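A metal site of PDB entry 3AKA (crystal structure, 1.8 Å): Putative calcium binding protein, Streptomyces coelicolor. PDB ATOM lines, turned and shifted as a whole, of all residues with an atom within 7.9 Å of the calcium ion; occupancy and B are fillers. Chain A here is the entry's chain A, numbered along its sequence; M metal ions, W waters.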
ATOM      1  N   PHE A  10      22.121  15.216  -0.358  1.00  0.00           N
ATOM      2  CA  PHE A  10      22.988  14.875   0.753  1.00  0.00           C
ATOM      3  C   PHE A  10      22.181  14.895   2.064  1.00  0.00           C
ATOM      4  O   PHE A  10      22.272  13.953   2.882  1.00  0.00           O
ATOM      5  CB  PHE A  10      24.174  15.826   0.843  1.00  0.00           C
ATOM      6  CG  PHE A  10      25.080  15.512   1.981  1.00  0.00           C
ATOM      7  CD1 PHE A  10      25.968  14.446   1.892  1.00  0.00           C
ATOM      8  CD2 PHE A  10      25.001  16.226   3.170  1.00  0.00           C
ATOM      9  CE1 PHE A  10      26.799  14.108   2.980  1.00  0.00           C
ATOM     10  CE2 PHE A  10      25.838  15.910   4.262  1.00  0.00           C
ATOM     11  CZ  PHE A  10      26.717  14.853   4.160  1.00  0.00           C
ATOM     12  N   THR A  11      21.394  15.949   2.240  1.00  0.00           N
ATOM     13  CA  THR A  11      20.564  16.148   3.438  1.00  0.00           C
ATOM     14  C   THR A  11      19.589  14.991   3.642  1.00  0.00           C
ATOM     15  O   THR A  11      19.346  14.577   4.783  1.00  0.00           O
ATOM     16  CB  THR A  11      19.848  17.531   3.428  1.00  0.00           C
ATOM     17  OG1 THR A  11      20.845  18.569   3.521  1.00  0.00           O
ATOM     18  CG2 THR A  11      18.901  17.668   4.623  1.00  0.00           C
ATOM     19  N   PHE A  13      20.132  11.809   2.928  1.00  0.00           N
ATOM     20  CA  PHE A  13      20.886  10.696   3.553  1.00  0.00           C
ATOM     21  C   PHE A  13      21.403  11.062   4.972  1.00  0.00           C
ATOM     22  O   PHE A  13      21.372  10.240   5.915  1.00  0.00           O
ATOM     23  CB  PHE A  13      22.065  10.296   2.656  1.00  0.00           C
ATOM     24  CG  PHE A  13      21.652   9.572   1.399  1.00  0.00           C
ATOM     25  CD1 PHE A  13      20.803   8.469   1.471  1.00  0.00           C
ATOM     26  CD2 PHE A  13      22.140   9.960   0.163  1.00  0.00           C
ATOM     27  CE1 PHE A  13      20.419   7.781   0.322  1.00  0.00           C
ATOM     28  CE2 PHE A  13      21.786   9.257  -0.998  1.00  0.00           C
ATOM     29  CZ  PHE A  13      20.911   8.180  -0.901  1.00  0.00           C
ATOM     30  N   ASP A  14      21.858  12.305   5.111  1.00  0.00           N
ATOM     31  CA  ASP A  14      22.330  12.826   6.396  1.00  0.00           C
ATOM     32  C   ASP A  14      21.135  13.172   7.305  1.00  0.00           C
ATOM     33  O   ASP A  14      20.884  14.335   7.646  1.00  0.00           O
ATOM     34  CB  ASP A  14      23.216  14.068   6.155  1.00  0.00           C
ATOM     35  CG  ASP A  14      23.847  14.568   7.432  1.00  0.00           C
ATOM     36  OD1 ASP A  14      23.965  13.784   8.419  1.00  0.00           O
ATOM     37  OD2 ASP A  14      24.270  15.754   7.449  1.00  0.00           O
ATOM     38  N   GLN A  15      20.402  12.130   7.709  1.00  0.00           N
ATOM     39  CA  GLN A  15      19.170  12.277   8.464  1.00  0.00           C
ATOM     40  C   GLN A  15      19.332  13.026   9.773  1.00  0.00           C
ATOM     41  O   GLN A  15      18.443  13.785  10.169  1.00  0.00           O
ATOM     42  CB  GLN A  15      18.551  10.911   8.716  1.00  0.00           C
ATOM     43  CG  GLN A  15      17.949  10.325   7.433  1.00  0.00           C
ATOM     44  CD  GLN A  15      16.558  10.872   7.182  1.00  0.00           C
ATOM     45  OE1 GLN A  15      15.731  10.900   8.071  1.00  0.00           O
ATOM     46  NE2 GLN A  15      16.295  11.285   5.948  1.00  0.00           N
ATOM     47  N   ASP A  16      20.465  12.816  10.445  1.00  0.00           N
ATOM     48  CA  ASP A  16      20.670  13.481  11.709  1.00  0.00           C
ATOM     49  C   ASP A  16      21.334  14.865  11.560  1.00  0.00           C
ATOM     50  O   ASP A  16      21.569  15.557  12.550  1.00  0.00           O
ATOM     51  CB  ASP A  16      21.365  12.549  12.731  1.00  0.00           C
ATOM     52  CG  ASP A  16      22.823  12.321  12.433  1.00  0.00           C
ATOM     53  OD1 ASP A  16      23.424  13.024  11.556  1.00  0.00           O
ATOM     54  OD2 ASP A  16      23.392  11.418  13.103  1.00  0.00           O
ATOM     55  N   GLY A  17      21.650  15.263  10.317  1.00  0.00           N
ATOM     56  CA  GLY A  17      22.142  16.636  10.052  1.00  0.00           C
ATOM     57  C   GLY A  17      23.584  16.982  10.457  1.00  0.00           C
ATOM     58  O   GLY A  17      23.994  18.167  10.395  1.00  0.00           O
ATOM     59  N   ASN A  18      24.369  15.977  10.825  1.00  0.00           N
ATOM     60  CA  ASN A  18      25.715  16.265  11.372  1.00  0.00           C
ATOM     61  C   ASN A  18      26.855  16.387  10.348  1.00  0.00           C
ATOM     62  O   ASN A  18      28.029  16.532  10.729  1.00  0.00           O
ATOM     63  CB  ASN A  18      26.093  15.295  12.513  1.00  0.00           C
ATOM     64  CG  ASN A  18      26.320  13.884  12.008  1.00  0.00           C
ATOM     65  OD1 ASN A  18      26.211  13.633  10.805  1.00  0.00           O
ATOM     66  ND2 ASN A  18      26.655  12.967  12.914  1.00  0.00           N
ATOM     67  N   GLY A  19      26.521  16.339   9.069  1.00  0.00           N
ATOM     68  CA  GLY A  19      27.469  16.639   7.978  1.00  0.00           C
ATOM     69  C   GLY A  19      28.256  15.464   7.390  1.00  0.00           C
ATOM     70  O   GLY A  19      29.067  15.616   6.454  1.00  0.00           O
ATOM     71  N   HIS A  20      28.020  14.270   7.927  1.00  0.00           N
ATOM     72  CA  HIS A  20      28.511  13.051   7.284  1.00  0.00           C
ATOM     73  C   HIS A  20      27.431  11.976   7.351  1.00  0.00           C
ATOM     74  O   HIS A  20      26.635  11.938   8.279  1.00  0.00           O
ATOM     75  CB  HIS A  20      29.834  12.531   7.917  1.00  0.00           C
ATOM     76  CG  HIS A  20      29.755  12.319   9.395  1.00  0.00           C
ATOM     77  ND1 HIS A  20      29.391  11.121   9.960  1.00  0.00           N
ATOM     78  CD2 HIS A  20      30.016  13.147  10.425  1.00  0.00           C
ATOM     79  CE1 HIS A  20      29.388  11.229  11.274  1.00  0.00           C
ATOM     80  NE2 HIS A  20      29.806  12.444  11.589  1.00  0.00           N
ATOM     81  N   ILE A  21      27.434  11.095   6.368  1.00  0.00           N
ATOM     82  CA  ILE A  21      26.481  10.003   6.361  1.00  0.00           C
ATOM     83  C   ILE A  21      27.153   8.804   7.048  1.00  0.00           C
ATOM     84  O   ILE A  21      28.271   8.442   6.653  1.00  0.00           O
ATOM     85  CB  ILE A  21      26.079   9.658   4.943  1.00  0.00           C
ATOM     86  CG1 ILE A  21      25.552  10.915   4.215  1.00  0.00           C
ATOM     87  CG2 ILE A  21      24.990   8.603   4.965  1.00  0.00           C
ATOM     88  CD1 ILE A  21      25.446  10.676   2.674  1.00  0.00           C
ATOM     89  N   ASP A  22      26.459   8.235   8.051  1.00  0.00           N
ATOM     90  CA  ASP A  22      26.871   7.099   8.916  1.00  0.00           C
ATOM     91  C   ASP A  22      25.818   5.979   8.723  1.00  0.00           C
ATOM     92  O   ASP A  22      24.685   6.259   8.343  1.00  0.00           O
ATOM     93  CB  ASP A  22      26.702   7.511  10.414  1.00  0.00           C
ATOM     94  CG  ASP A  22      27.907   8.210  10.993  1.00  0.00           C
ATOM     95  OD1 ASP A  22      29.030   8.084  10.466  1.00  0.00           O
ATOM     96  OD2 ASP A  22      27.746   8.930  12.016  1.00  0.00           O
ATOM     97  N   ARG A  23      26.135   4.735   9.102  1.00  0.00           N
ATOM     98  CA  ARG A  23      25.098   3.679   9.248  1.00  0.00           C
ATOM     99  C   ARG A  23      23.959   4.178  10.166  1.00  0.00           C
ATOM    100  O   ARG A  23      22.782   3.910   9.914  1.00  0.00           O
ATOM    101  CB  ARG A  23      25.730   2.350   9.785  1.00  0.00           C
ATOM    102  CG  ARG A  23      24.767   1.125   9.872  1.00  0.00           C
ATOM    103  CD  ARG A  23      25.532  -0.209  10.136  1.00  0.00           C
ATOM    104  NE  ARG A  23      25.578  -0.774  11.506  1.00  0.00           N
ATOM    105  CZ  ARG A  23      25.102  -0.214  12.619  1.00  0.00           C
ATOM    106  NH1 ARG A  23      24.497   0.976  12.582  1.00  0.00           N
ATOM    107  NH2 ARG A  23      25.219  -0.857  13.775  1.00  0.00           N
ATOM    108  N   SER A  24      24.292   4.938  11.207  1.00  0.00           N
ATOM    109  CA  SER A  24      23.245   5.352  12.151  1.00  0.00           C
ATOM    110  C   SER A  24      22.219   6.314  11.546  1.00  0.00           C
ATOM    111  O   SER A  24      21.108   6.412  12.054  1.00  0.00           O
ATOM    112  CB  SER A  24      23.837   5.936  13.430  1.00  0.00           C
ATOM    113  OG  SER A  24      24.622   7.038  13.123  1.00  0.00           O
ATOM    114  N   ASP A  25      22.586   7.055  10.494  1.00  0.00           N
ATOM    115  CA  ASP A  25      21.618   7.895   9.795  1.00  0.00           C
ATOM    116  C   ASP A  25      20.509   6.980   9.267  1.00  0.00           C
ATOM    117  O   ASP A  25      19.320   7.309   9.370  1.00  0.00           O
ATOM    118  CB  ASP A  25      22.265   8.649   8.618  1.00  0.00           C
ATOM    119  CG  ASP A  25      23.019   9.875   9.074  1.00  0.00           C
ATOM    120  OD1 ASP A  25      22.458  10.705   9.836  1.00  0.00           O
ATOM    121  OD2 ASP A  25      24.204   9.983   8.702  1.00  0.00           O
ATOM    122  N   PHE A  26      20.936   5.861   8.662  1.00  0.00           N
ATOM    123  CA  PHE A  26      19.998   4.875   8.116  1.00  0.00           C
ATOM    124  C   PHE A  26      19.198   4.145   9.197  1.00  0.00           C
ATOM    125  O   PHE A  26      17.982   4.002   9.077  1.00  0.00           O
ATOM    126  CB  PHE A  26      20.729   3.894   7.201  1.00  0.00           C
ATOM    127  CG  PHE A  26      21.145   4.503   5.902  1.00  0.00           C
ATOM    128  CD1 PHE A  26      20.337   4.388   4.770  1.00  0.00           C
ATOM    129  CD2 PHE A  26      22.328   5.231   5.816  1.00  0.00           C
ATOM    130  CE1 PHE A  26      20.734   4.973   3.537  1.00  0.00           C
ATOM    131  CE2 PHE A  26      22.737   5.798   4.618  1.00  0.00           C
ATOM    132  CZ  PHE A  26      21.933   5.683   3.476  1.00  0.00           C
ATOM    133  N   ILE A  72      30.461   9.054   5.289  1.00  0.00           N
ATOM    134  CA  ILE A  72      30.561   9.706   3.976  1.00  0.00           C
ATOM    135  C   ILE A  72      30.423  11.205   4.221  1.00  0.00           C
ATOM    136  O   ILE A  72      29.355  11.658   4.640  1.00  0.00           O
ATOM    137  CB  ILE A  72      29.414   9.222   3.071  1.00  0.00           C
ATOM    138  CG1 ILE A  72      29.395   7.683   2.981  1.00  0.00           C
ATOM    139  CG2 ILE A  72      29.464   9.947   1.682  1.00  0.00           C
ATOM    140  CD1 ILE A  72      28.249   7.108   2.060  1.00  0.00           C
HETATM  141 CA    CA M   1      24.711  12.006   9.815  1.00  0.00          CA
HETATM  142  O   HOH W   1      25.357  10.524  11.632  1.00  0.00           O
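Five residues have an atom within 4 Å of the calcium ion: Asp 14, Asp 16, Asn 18, His 20 and Asp 25.
The calcium ion is bound by the side-chain carboxylate (OD2) of Asp 25 (2.4 Å), the side-chain carboxylate (OD1) of Asp 14 (2.4 Å), the side-chain carboxylate (OD1) of Asp 16 (2.4 Å), the side-chain amide oxygen (OD1) of Asn 18 (2.4 Å), water W1 (2.4 Å), the backbone carbonyl oxygen (O) of His 20 (2.5 Å) and the side-chain carboxylate (OD1) of Asp 25 (2.6 Å).
Water W1 lies within hydrogen-bond range of OD2 of Asp 16 (2.6 Å), OD2 of Asp 22 (2.9 Å) and ND2 of Asn 18 (3.0 Å).
OD2 of Asp 25 sits close to N of Asp 22, 2.9 Å away.
The side-chain carboxylate of Asp 25 sits close to the backbone NH of Gln 15 (3.3 Å).
The side-chain carboxylate (OD1) of Asp 14 lies close to the backbone NH (N) of Gly 17.
The side-chain carboxylate of Asp 14 sits at hydrogen-bond distance from the backbone NH of Gly 19 (2.8 Å).
OD1 of Asp 22 is in hydrogen-bond range of ND1 of His 20 (3.1 Å).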
